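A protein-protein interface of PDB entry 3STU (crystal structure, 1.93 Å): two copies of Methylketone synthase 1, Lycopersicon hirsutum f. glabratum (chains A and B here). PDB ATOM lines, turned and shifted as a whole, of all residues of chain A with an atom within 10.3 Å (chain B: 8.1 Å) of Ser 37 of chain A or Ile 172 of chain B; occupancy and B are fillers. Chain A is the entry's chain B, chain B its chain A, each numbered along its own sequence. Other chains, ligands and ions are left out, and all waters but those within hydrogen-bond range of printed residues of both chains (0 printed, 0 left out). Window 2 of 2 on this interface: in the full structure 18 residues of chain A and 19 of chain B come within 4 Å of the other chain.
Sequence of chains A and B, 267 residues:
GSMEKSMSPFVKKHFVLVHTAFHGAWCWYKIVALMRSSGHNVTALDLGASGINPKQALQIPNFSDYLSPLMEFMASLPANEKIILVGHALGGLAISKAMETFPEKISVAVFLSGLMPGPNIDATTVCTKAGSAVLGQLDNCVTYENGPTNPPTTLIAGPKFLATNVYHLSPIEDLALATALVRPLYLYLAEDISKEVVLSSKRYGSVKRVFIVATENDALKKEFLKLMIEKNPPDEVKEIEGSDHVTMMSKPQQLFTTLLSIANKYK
Position printed for both chains: 30.
OG1 of Thr 179 of chain B is in hydrogen-bond range of NH1 of Arg 36 of chain A (3.2 Å).
Of chain B, only Ile 172 comes within 4 Å of Ser 37 of chain A. Ile 172 of chain B touches two residues of chain A. Of chain A, only Tyr 29 and Ala 33 come within 4 Å of Glu 173 of chain B. No residue of chain A comes within 4 Å of Leu 175 of chain B. Of the printed residues of chain A, Thr 179 of chain B touches Arg 36 (3.2 Å). Printed residues of chain A within 4 Å of Leu 177 of chain B: Tyr 29. Of the printed residues of chain A, Ala 176 of chain B touches Tyr 29 (3.6 Å) and Val 32 (3.8 Å). Printed residues of chain B within 4 Å of Tyr 29 of chain A: Glu 173, Ala 176 and Leu 177. Printed residues of chain B within 4 Å of Val 32 of chain A: Ala 176. Leu 34 of chain A touches none of the printed residues of chain B. Trp 28 of chain A touches none of the printed residues of chain B. The nearest residue of chain A that does not touch Ile 172 of chain B is Leu 34 of chain A (4.8 Å).
Hydrophobic or aromatic side chains of chain B that line the printed part of chain A: Ile 172, Ala 176 and Leu 177. Among the printed residues, no Asp or Glu carboxylate lies within 4 Å of a Lys or Arg side-chain nitrogen of the other chain.
The backbone carbonyl oxygen (O) of Ala 176 of chain B sits at hydrogen-bond distance from the side-chain hydroxyl (OG1) of Thr 179 of chain B, at 2.6 Å. O of Leu 175 of chain B lies close to OG1 of Thr 179 of chain B.
Among the printed residues, merely in contact across the chains: Tyr 29 of chain A with Glu 173 of chain B, Tyr 29 of chain A with Ala 176 of chain B, Ala 33 of chain A with Glu 173 of chain B, Tyr 29 of chain A with Leu 177 of chain B, Val 32 of chain A with Ala 176 of chain B, Ala 33 of chain A with Ile 172 of chain B and Ser 37 of chain A with Ile 172 of chain B.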
ATOM      1  N   PHE A  10      12.557  -3.565  -4.386  1.00  0.00           N
ATOM      2  CA  PHE A  10      11.855  -2.403  -4.949  1.00  0.00           C
ATOM      3  C   PHE A  10      12.805  -1.326  -5.467  1.00  0.00           C
ATOM      4  O   PHE A  10      13.682  -0.860  -4.742  1.00  0.00           O
ATOM      5  CB  PHE A  10      10.869  -1.801  -3.930  1.00  0.00           C
ATOM      6  CG  PHE A  10       9.995  -0.699  -4.496  1.00  0.00           C
ATOM      7  CD1 PHE A  10      10.286   0.643  -4.245  1.00  0.00           C
ATOM      8  CD2 PHE A  10       8.883  -1.005  -5.283  1.00  0.00           C
ATOM      9  CE1 PHE A  10       9.486   1.661  -4.771  1.00  0.00           C
ATOM     10  CE2 PHE A  10       8.076   0.005  -5.813  1.00  0.00           C
ATOM     11  CZ  PHE A  10       8.376   1.339  -5.557  1.00  0.00           C
ATOM     12  N   LYS A  12      12.369   2.395  -7.138  1.00  0.00           N
ATOM     13  CA  LYS A  12      11.454   3.494  -7.455  1.00  0.00           C
ATOM     14  C   LYS A  12      11.662   4.017  -8.876  1.00  0.00           C
ATOM     15  O   LYS A  12      12.786   4.329  -9.288  1.00  0.00           O
ATOM     16  CB  LYS A  12      11.603   4.631  -6.446  1.00  0.00           C
ATOM     17  CG  LYS A  12      10.470   5.634  -6.484  1.00  0.00           C
ATOM     18  CD  LYS A  12      10.727   6.799  -5.544  1.00  0.00           C
ATOM     19  CE  LYS A  12       9.508   7.700  -5.460  1.00  0.00           C
ATOM     20  NZ  LYS A  12       9.847   9.043  -4.913  1.00  0.00           N
ATOM     21  N   PHE A  15       7.327   7.282 -14.039  1.00  0.00           N
ATOM     22  CA  PHE A  15       6.493   7.158 -15.228  1.00  0.00           C
ATOM     23  C   PHE A  15       5.955   8.526 -15.648  1.00  0.00           C
ATOM     24  O   PHE A  15       5.467   9.293 -14.816  1.00  0.00           O
ATOM     25  CB  PHE A  15       5.323   6.192 -14.982  1.00  0.00           C
ATOM     26  CG  PHE A  15       5.745   4.773 -14.714  1.00  0.00           C
ATOM     27  CD1 PHE A  15       5.937   3.881 -15.768  1.00  0.00           C
ATOM     28  CD2 PHE A  15       5.927   4.323 -13.407  1.00  0.00           C
ATOM     29  CE1 PHE A  15       6.326   2.553 -15.528  1.00  0.00           C
ATOM     30  CE2 PHE A  15       6.310   2.996 -13.147  1.00  0.00           C
ATOM     31  CZ  PHE A  15       6.515   2.111 -14.215  1.00  0.00           C
ATOM     32  N   TRP A  28      -5.667   9.357 -17.408  1.00  0.00           N
ATOM     33  CA  TRP A  28      -4.769   8.386 -16.800  1.00  0.00           C
ATOM     34  C   TRP A  28      -5.067   8.108 -15.326  1.00  0.00           C
ATOM     35  O   TRP A  28      -4.288   7.412 -14.675  1.00  0.00           O
ATOM     36  CB  TRP A  28      -3.318   8.866 -16.909  1.00  0.00           C
ATOM     37  CG  TRP A  28      -2.782   9.008 -18.310  1.00  0.00           C
ATOM     38  CD1 TRP A  28      -2.654  10.172 -19.027  1.00  0.00           C
ATOM     39  CD2 TRP A  28      -2.262   7.964 -19.145  1.00  0.00           C
ATOM     40  NE1 TRP A  28      -2.100   9.909 -20.262  1.00  0.00           N
ATOM     41  CE2 TRP A  28      -1.851   8.565 -20.362  1.00  0.00           C
ATOM     42  CE3 TRP A  28      -2.112   6.579 -18.991  1.00  0.00           C
ATOM     43  CZ2 TRP A  28      -1.291   7.824 -21.419  1.00  0.00           C
ATOM     44  CZ3 TRP A  28      -1.550   5.842 -20.044  1.00  0.00           C
ATOM     45  CH2 TRP A  28      -1.151   6.467 -21.239  1.00  0.00           C
ATOM     46  N   TYR A  29      -6.176   8.628 -14.804  1.00  0.00           N
ATOM     47  CA  TYR A  29      -6.436   8.592 -13.344  1.00  0.00           C
ATOM     48  C   TYR A  29      -6.359   7.218 -12.668  1.00  0.00           C
ATOM     49  O   TYR A  29      -5.878   7.113 -11.537  1.00  0.00           O
ATOM     50  CB  TYR A  29      -7.740   9.305 -12.985  1.00  0.00           C
ATOM     51  CG  TYR A  29      -9.021   8.540 -13.252  1.00  0.00           C
ATOM     52  CD1 TYR A  29      -9.766   8.020 -12.192  1.00  0.00           C
ATOM     53  CD2 TYR A  29      -9.504   8.363 -14.556  1.00  0.00           C
ATOM     54  CE1 TYR A  29     -10.962   7.337 -12.418  1.00  0.00           C
ATOM     55  CE2 TYR A  29     -10.690   7.677 -14.793  1.00  0.00           C
ATOM     56  CZ  TYR A  29     -11.414   7.170 -13.718  1.00  0.00           C
ATOM     57  OH  TYR A  29     -12.596   6.505 -13.936  1.00  0.00           O
ATOM     58  N   LYS A  30      -6.833   6.178 -13.354  1.00  0.00           N
ATOM     59  CA  LYS A  30      -6.767   4.828 -12.790  1.00  0.00           C
ATOM     60  C   LYS A  30      -5.320   4.342 -12.713  1.00  0.00           C
ATOM     61  O   LYS A  30      -4.943   3.697 -11.745  1.00  0.00           O
ATOM     62  CB  LYS A  30      -7.619   3.846 -13.589  1.00  0.00           C
ATOM     63  CG  LYS A  30      -9.089   4.213 -13.656  1.00  0.00           C
ATOM     64  CD  LYS A  30      -9.815   3.301 -14.638  1.00  0.00           C
ATOM     65  CE  LYS A  30     -11.290   3.637 -14.709  1.00  0.00           C
ATOM     66  NZ  LYS A  30     -12.023   2.709 -15.612  1.00  0.00           N
ATOM     67  N   ILE A  31      -4.523   4.665 -13.729  1.00  0.00           N
ATOM     68  CA  ILE A  31      -3.111   4.265 -13.778  1.00  0.00           C
ATOM     69  C   ILE A  31      -2.294   5.053 -12.751  1.00  0.00           C
ATOM     70  O   ILE A  31      -1.436   4.497 -12.059  1.00  0.00           O
ATOM     71  CB  ILE A  31      -2.509   4.464 -15.200  1.00  0.00           C
ATOM     72  CG1 ILE A  31      -3.356   3.748 -16.274  1.00  0.00           C
ATOM     73  CG2 ILE A  31      -1.033   4.032 -15.246  1.00  0.00           C
ATOM     74  CD1 ILE A  31      -3.558   2.256 -16.045  1.00  0.00           C
ATOM     75  N   VAL A  32      -2.571   6.348 -12.664  1.00  0.00           N
ATOM     76  CA  VAL A  32      -1.920   7.227 -11.697  1.00  0.00           C
ATOM     77  C   VAL A  32      -2.103   6.734 -10.258  1.00  0.00           C
ATOM     78  O   VAL A  32      -1.143   6.714  -9.476  1.00  0.00           O
ATOM     79  CB  VAL A  32      -2.402   8.689 -11.857  1.00  0.00           C
ATOM     80  CG1 VAL A  32      -1.989   9.533 -10.658  1.00  0.00           C
ATOM     81  CG2 VAL A  32      -1.837   9.290 -13.163  1.00  0.00           C
ATOM     82  N   ALA A  33      -3.325   6.329  -9.918  1.00  0.00           N
ATOM     83  CA  ALA A  33      -3.620   5.828  -8.575  1.00  0.00           C
ATOM     84  C   ALA A  33      -2.847   4.538  -8.289  1.00  0.00           C
ATOM     85  O   ALA A  33      -2.279   4.384  -7.212  1.00  0.00           O
ATOM     86  CB  ALA A  33      -5.111   5.602  -8.407  1.00  0.00           C
ATOM     87  N   LEU A  34      -2.823   3.622  -9.256  1.00  0.00           N
ATOM     88  CA  LEU A  34      -2.092   2.363  -9.105  1.00  0.00           C
ATOM     89  C   LEU A  34      -0.581   2.599  -8.914  1.00  0.00           C
ATOM     90  O   LEU A  34       0.060   1.955  -8.081  1.00  0.00           O
ATOM     91  CB  LEU A  34      -2.363   1.434 -10.294  1.00  0.00           C
ATOM     92  CG  LEU A  34      -3.790   0.858 -10.389  1.00  0.00           C
ATOM     93  CD1 LEU A  34      -4.035   0.165 -11.720  1.00  0.00           C
ATOM     94  CD2 LEU A  34      -4.088  -0.096  -9.229  1.00  0.00           C
ATOM     95  N   MET A  35      -0.028   3.538  -9.671  1.00  0.00           N
ATOM     96  CA  MET A  35       1.391   3.881  -9.554  1.00  0.00           C
ATOM     97  C   MET A  35       1.741   4.558  -8.229  1.00  0.00           C
ATOM     98  O   MET A  35       2.736   4.199  -7.595  1.00  0.00           O
ATOM     99  CB  MET A  35       1.830   4.738 -10.737  1.00  0.00           C
ATOM    100  CG  MET A  35       2.147   3.916 -11.963  1.00  0.00           C
ATOM    101  SD  MET A  35       2.140   4.882 -13.475  1.00  0.00           S
ATOM    102  CE  MET A  35       2.482   3.574 -14.653  1.00  0.00           C
ATOM    103  N   ARG A  36       0.928   5.525  -7.812  1.00  0.00           N
ATOM    104  CA  ARG A  36       1.174   6.254  -6.560  1.00  0.00           C
ATOM    105  C   ARG A  36       0.995   5.364  -5.339  1.00  0.00           C
ATOM    106  O   ARG A  36       1.698   5.529  -4.345  1.00  0.00           O
ATOM    107  CB  ARG A  36       0.273   7.485  -6.444  1.00  0.00           C
ATOM    108  CG  ARG A  36       0.767   8.689  -7.216  1.00  0.00           C
ATOM    109  CD  ARG A  36      -0.268   9.798  -7.220  1.00  0.00           C
ATOM    110  NE  ARG A  36       0.128  10.910  -8.077  1.00  0.00           N
ATOM    111  CZ  ARG A  36      -0.675  11.905  -8.452  1.00  0.00           C
ATOM    112  NH1 ARG A  36      -1.939  11.942  -8.055  1.00  0.00           N
ATOM    113  NH2 ARG A  36      -0.211  12.868  -9.235  1.00  0.00           N
ATOM    114  N   SER A  37       0.054   4.427  -5.426  1.00  0.00           N
ATOM    115  CA  SER A  37      -0.214   3.484  -4.343  1.00  0.00           C
ATOM    116  C   SER A  37       0.954   2.523  -4.118  1.00  0.00           C
ATOM    117  O   SER A  37       1.215   2.120  -2.986  1.00  0.00           O
ATOM    118  CB  SER A  37      -1.501   2.702  -4.615  1.00  0.00           C
ATOM    119  OG  SER A  37      -1.621   1.613  -3.718  1.00  0.00           O
ATOM    120  N   SER A  38       1.654   2.158  -5.189  1.00  0.00           N
ATOM    121  CA  SER A  38       2.809   1.266  -5.058  1.00  0.00           C
ATOM    122  C   SER A  38       4.144   1.979  -4.841  1.00  0.00           C
ATOM    123  O   SER A  38       5.183   1.332  -4.769  1.00  0.00           O
ATOM    124  CB  SER A  38       2.897   0.275  -6.225  1.00  0.00           C
ATOM    125  OG  SER A  38       2.376   0.808  -7.424  1.00  0.00           O
ATOM    126  N   GLY A  39       4.115   3.303  -4.726  1.00  0.00           N
ATOM    127  CA  GLY A  39       5.312   4.071  -4.384  1.00  0.00           C
ATOM    128  C   GLY A  39       6.169   4.556  -5.542  1.00  0.00           C
ATOM    129  O   GLY A  39       7.295   5.027  -5.330  1.00  0.00           O
ATOM    130  N   HIS A  40       5.656   4.453  -6.766  1.00  0.00           N
ATOM    131  CA  HIS A  40       6.386   4.968  -7.923  1.00  0.00           C
ATOM    132  C   HIS A  40       6.063   6.439  -8.161  1.00  0.00           C
ATOM    133  O   HIS A  40       4.991   6.913  -7.772  1.00  0.00           O
ATOM    134  CB  HIS A  40       6.071   4.172  -9.192  1.00  0.00           C
ATOM    135  CG  HIS A  40       6.542   2.751  -9.157  1.00  0.00           C
ATOM    136  ND1 HIS A  40       7.877   2.408  -9.139  1.00  0.00           N
ATOM    137  CD2 HIS A  40       5.853   1.584  -9.157  1.00  0.00           C
ATOM    138  CE1 HIS A  40       7.990   1.091  -9.123  1.00  0.00           C
ATOM    139  NE2 HIS A  40       6.776   0.569  -9.130  1.00  0.00           N
ATOM    140  N   ASN A  41       7.005   7.154  -8.778  1.00  0.00           N
ATOM    141  CA  ASN A  41       6.741   8.513  -9.222  1.00  0.00           C
ATOM    142  C   ASN A  41       6.002   8.489 -10.554  1.00  0.00           C
ATOM    143  O   ASN A  41       6.318   7.698 -11.445  1.00  0.00           O
ATOM    144  CB  ASN A  41       8.035   9.313  -9.344  1.00  0.00           C
ATOM    145  CG  ASN A  41       7.800  10.810  -9.305  1.00  0.00           C
ATOM    146  OD1 ASN A  41       6.684  11.273  -9.057  1.00  0.00           O
ATOM    147  ND2 ASN A  41       8.858  11.580  -9.543  1.00  0.00           N
ATOM    148  N   VAL A  42       5.002   9.348 -10.673  1.00  0.00           N
ATOM    149  CA  VAL A  42       4.214   9.444 -11.893  1.00  0.00           C
ATOM    150  C   VAL A  42       3.825  10.900 -12.142  1.00  0.00           C
ATOM    151  O   VAL A  42       3.364  11.596 -11.236  1.00  0.00           O
ATOM    152  CB  VAL A  42       2.979   8.483 -11.875  1.00  0.00           C
ATOM    153  CG1 VAL A  42       2.171   8.623 -10.580  1.00  0.00           C
ATOM    154  CG2 VAL A  42       2.097   8.676 -13.113  1.00  0.00           C
ATOM    155  N   GLN A 253      -5.792  -2.355 -14.993  1.00  0.00           N
ATOM    156  CA  GLN A 253      -4.906  -3.188 -14.176  1.00  0.00           C
ATOM    157  C   GLN A 253      -3.887  -3.917 -15.063  1.00  0.00           C
ATOM    158  O   GLN A 253      -2.706  -4.005 -14.722  1.00  0.00           O
ATOM    159  CB  GLN A 253      -5.723  -4.153 -13.305  1.00  0.00           C
ATOM    160  CG  GLN A 253      -4.911  -4.958 -12.264  1.00  0.00           C
ATOM    161  CD  GLN A 253      -4.248  -4.103 -11.170  1.00  0.00           C
ATOM    162  OE1 GLN A 253      -4.877  -3.224 -10.568  1.00  0.00           O
ATOM    163  NE2 GLN A 253      -2.976  -4.378 -10.904  1.00  0.00           N
ATOM    164  N   PHE A 256      -1.282  -1.484 -16.231  1.00  0.00           N
ATOM    165  CA  PHE A 256      -0.384  -1.213 -15.110  1.00  0.00           C
ATOM    166  C   PHE A 256       0.702  -2.281 -14.943  1.00  0.00           C
ATOM    167  O   PHE A 256       1.894  -1.964 -14.891  1.00  0.00           O
ATOM    168  CB  PHE A 256      -1.198  -1.062 -13.824  1.00  0.00           C
ATOM    169  CG  PHE A 256      -0.363  -0.937 -12.582  1.00  0.00           C
ATOM    170  CD1 PHE A 256       0.431   0.185 -12.371  1.00  0.00           C
ATOM    171  CD2 PHE A 256      -0.392  -1.935 -11.609  1.00  0.00           C
ATOM    172  CE1 PHE A 256       1.192   0.303 -11.208  1.00  0.00           C
ATOM    173  CE2 PHE A 256       0.365  -1.824 -10.452  1.00  0.00           C
ATOM    174  CZ  PHE A 256       1.155  -0.705 -10.249  1.00  0.00           C
ATOM    175  N   LEU A 260       4.813  -1.902 -15.511  1.00  0.00           N
ATOM    176  CA  LEU A 260       5.810  -2.289 -14.501  1.00  0.00           C
ATOM    177  C   LEU A 260       6.831  -3.286 -15.056  1.00  0.00           C
ATOM    178  O   LEU A 260       8.031  -3.174 -14.798  1.00  0.00           O
ATOM    179  CB  LEU A 260       5.135  -2.885 -13.267  1.00  0.00           C
ATOM    180  CG  LEU A 260       4.256  -2.022 -12.353  1.00  0.00           C
ATOM    181  CD1 LEU A 260       3.896  -2.845 -11.116  1.00  0.00           C
ATOM    182  CD2 LEU A 260       4.926  -0.710 -11.936  1.00  0.00           C
ATOM    183  N   LYS B  30     -20.152   9.676 -12.098  1.00  0.00           N
ATOM    184  CA  LYS B  30     -20.812   8.430 -11.682  1.00  0.00           C
ATOM    185  C   LYS B  30     -22.323   8.598 -11.685  1.00  0.00           C
ATOM    186  O   LYS B  30     -23.059   7.705 -12.117  1.00  0.00           O
ATOM    187  CB  LYS B  30     -20.331   7.998 -10.298  1.00  0.00           C
ATOM    188  CG  LYS B  30     -18.872   7.604 -10.267  1.00  0.00           C
ATOM    189  CD  LYS B  30     -18.444   7.220  -8.873  1.00  0.00           C
ATOM    190  CE  LYS B  30     -16.927   7.202  -8.755  1.00  0.00           C
ATOM    191  NZ  LYS B  30     -16.538   6.762  -7.378  1.00  0.00           N
ATOM    192  N   TYR B 167     -11.716  13.729   0.081  1.00  0.00           N
ATOM    193  CA  TYR B 167     -11.840  12.421  -0.582  1.00  0.00           C
ATOM    194  C   TYR B 167     -11.559  11.218   0.318  1.00  0.00           C
ATOM    195  O   TYR B 167     -11.355  10.103  -0.173  1.00  0.00           O
ATOM    196  CB  TYR B 167     -10.925  12.375  -1.810  1.00  0.00           C
ATOM    197  CG  TYR B 167     -11.486  13.126  -2.991  1.00  0.00           C
ATOM    198  CD1 TYR B 167     -11.415  14.517  -3.053  1.00  0.00           C
ATOM    199  CD2 TYR B 167     -12.098  12.445  -4.045  1.00  0.00           C
ATOM    200  CE1 TYR B 167     -11.945  15.216  -4.136  1.00  0.00           C
ATOM    201  CE2 TYR B 167     -12.626  13.136  -5.141  1.00  0.00           C
ATOM    202  CZ  TYR B 167     -12.544  14.521  -5.172  1.00  0.00           C
ATOM    203  OH  TYR B 167     -13.064  15.220  -6.240  1.00  0.00           O
ATOM    204  N   LEU B 169     -13.123   9.104   2.109  1.00  0.00           N
ATOM    205  CA  LEU B 169     -13.913   7.862   2.012  1.00  0.00           C
ATOM    206  C   LEU B 169     -14.169   7.408   0.563  1.00  0.00           C
ATOM    207  O   LEU B 169     -14.998   6.527   0.305  1.00  0.00           O
ATOM    208  CB  LEU B 169     -15.232   7.986   2.797  1.00  0.00           C
ATOM    209  CG  LEU B 169     -15.108   8.177   4.318  1.00  0.00           C
ATOM    210  CD1 LEU B 169     -16.459   8.426   4.994  1.00  0.00           C
ATOM    211  CD2 LEU B 169     -14.371   7.010   4.982  1.00  0.00           C
ATOM    212  N   SER B 170     -13.445   8.004  -0.379  1.00  0.00           N
ATOM    213  CA  SER B 170     -13.628   7.712  -1.799  1.00  0.00           C
ATOM    214  C   SER B 170     -12.540   6.763  -2.325  1.00  0.00           C
ATOM    215  O   SER B 170     -11.467   6.679  -1.733  1.00  0.00           O
ATOM    216  CB  SER B 170     -13.636   9.019  -2.602  1.00  0.00           C
ATOM    217  OG  SER B 170     -14.794   9.782  -2.290  1.00  0.00           O
ATOM    218  N   PRO B 171     -12.811   6.047  -3.438  1.00  0.00           N
ATOM    219  CA  PRO B 171     -11.759   5.227  -4.059  1.00  0.00           C
ATOM    220  C   PRO B 171     -10.522   6.062  -4.393  1.00  0.00           C
ATOM    221  O   PRO B 171     -10.646   7.244  -4.709  1.00  0.00           O
ATOM    222  CB  PRO B 171     -12.420   4.716  -5.344  1.00  0.00           C
ATOM    223  CG  PRO B 171     -13.885   4.734  -5.046  1.00  0.00           C
ATOM    224  CD  PRO B 171     -14.109   5.899  -4.126  1.00  0.00           C
ATOM    225  N   ILE B 172      -9.343   5.453  -4.309  1.00  0.00           N
ATOM    226  CA  ILE B 172      -8.089   6.194  -4.504  1.00  0.00           C
ATOM    227  C   ILE B 172      -7.957   6.791  -5.904  1.00  0.00           C
ATOM    228  O   ILE B 172      -7.298   7.819  -6.085  1.00  0.00           O
ATOM    229  CB  ILE B 172      -6.821   5.353  -4.156  1.00  0.00           C
ATOM    230  CG1 ILE B 172      -6.787   4.033  -4.942  1.00  0.00           C
ATOM    231  CG2 ILE B 172      -6.741   5.118  -2.653  1.00  0.00           C
ATOM    232  CD1 ILE B 172      -5.367   3.459  -5.145  1.00  0.00           C
ATOM    233  N   GLU B 173      -8.595   6.161  -6.891  1.00  0.00           N
ATOM    234  CA  GLU B 173      -8.550   6.693  -8.251  1.00  0.00           C
ATOM    235  C   GLU B 173      -9.299   8.029  -8.388  1.00  0.00           C
ATOM    236  O   GLU B 173      -8.915   8.868  -9.198  1.00  0.00           O
ATOM    237  CB  GLU B 173      -9.005   5.656  -9.298  1.00  0.00           C
ATOM    238  CG  GLU B 173     -10.470   5.222  -9.213  1.00  0.00           C
ATOM    239  CD  GLU B 173     -10.693   3.970  -8.357  1.00  0.00           C
ATOM    240  OE1 GLU B 173     -11.705   3.266  -8.607  1.00  0.00           O
ATOM    241  OE2 GLU B 173      -9.876   3.687  -7.439  1.00  0.00           O
ATOM    242  N   ASP B 174     -10.346   8.235  -7.588  1.00  0.00           N
ATOM    243  CA  ASP B 174     -11.094   9.502  -7.638  1.00  0.00           C
ATOM    244  C   ASP B 174     -10.291  10.654  -7.047  1.00  0.00           C
ATOM    245  O   ASP B 174     -10.407  11.804  -7.493  1.00  0.00           O
ATOM    246  CB  ASP B 174     -12.461   9.365  -6.964  1.00  0.00           C
ATOM    247  CG  ASP B 174     -13.382   8.391  -7.706  1.00  0.00           C
ATOM    248  OD1 ASP B 174     -13.378   8.394  -8.956  1.00  0.00           O
ATOM    249  OD2 ASP B 174     -14.107   7.628  -7.044  1.00  0.00           O
ATOM    250  N   LEU B 175      -9.465  10.338  -6.049  1.00  0.00           N
ATOM    251  CA  LEU B 175      -8.490  11.295  -5.559  1.00  0.00           C
ATOM    252  C   LEU B 175      -7.501  11.668  -6.664  1.00  0.00           C
ATOM    253  O   LEU B 175      -7.225  12.848  -6.857  1.00  0.00           O
ATOM    254  CB  LEU B 175      -7.762  10.778  -4.306  1.00  0.00           C
ATOM    255  CG  LEU B 175      -6.570  11.602  -3.794  1.00  0.00           C
ATOM    256  CD1 LEU B 175      -6.968  13.035  -3.401  1.00  0.00           C
ATOM    257  CD2 LEU B 175      -5.938  10.876  -2.627  1.00  0.00           C
ATOM    258  N   ALA B 176      -6.984  10.675  -7.393  1.00  0.00           N
ATOM    259  CA  ALA B 176      -6.040  10.958  -8.481  1.00  0.00           C
ATOM    260  C   ALA B 176      -6.693  11.807  -9.565  1.00  0.00           C
ATOM    261  O   ALA B 176      -6.075  12.741 -10.074  1.00  0.00           O
ATOM    262  CB  ALA B 176      -5.464   9.672  -9.080  1.00  0.00           C
ATOM    263  N   LEU B 177      -7.944  11.482  -9.893  1.00  0.00           N
ATOM    264  CA  LEU B 177      -8.735  12.241 -10.867  1.00  0.00           C
ATOM    265  C   LEU B 177      -8.862  13.707 -10.457  1.00  0.00           C
ATOM    266  O   LEU B 177      -8.624  14.618 -11.263  1.00  0.00           O
ATOM    267  CB  LEU B 177     -10.127  11.604 -11.038  1.00  0.00           C
ATOM    268  CG  LEU B 177     -11.082  12.216 -12.076  1.00  0.00           C
ATOM    269  CD1 LEU B 177     -10.493  12.143 -13.493  1.00  0.00           C
ATOM    270  CD2 LEU B 177     -12.455  11.531 -12.036  1.00  0.00           C
ATOM    271  N   ALA B 178      -9.213  13.922  -9.190  1.00  0.00           N
ATOM    272  CA  ALA B 178      -9.358  15.260  -8.636  1.00  0.00           C
ATOM    273  C   ALA B 178      -8.056  16.039  -8.671  1.00  0.00           C
ATOM    274  O   ALA B 178      -8.046  17.220  -9.021  1.00  0.00           O
ATOM    275  CB  ALA B 178      -9.883  15.192  -7.215  1.00  0.00           C
ATOM    276  N   THR B 179      -6.959  15.378  -8.309  1.00  0.00           N
ATOM    277  CA  THR B 179      -5.663  16.042  -8.295  1.00  0.00           C
ATOM    278  C   THR B 179      -5.280  16.548  -9.683  1.00  0.00           C
ATOM    279  O   THR B 179      -4.582  17.552  -9.791  1.00  0.00           O
ATOM    280  CB  THR B 179      -4.548  15.164  -7.689  1.00  0.00           C
ATOM    281  OG1 THR B 179      -4.429  13.949  -8.438  1.00  0.00           O
ATOM    282  CG2 THR B 179      -4.858  14.836  -6.232  1.00  0.00           C
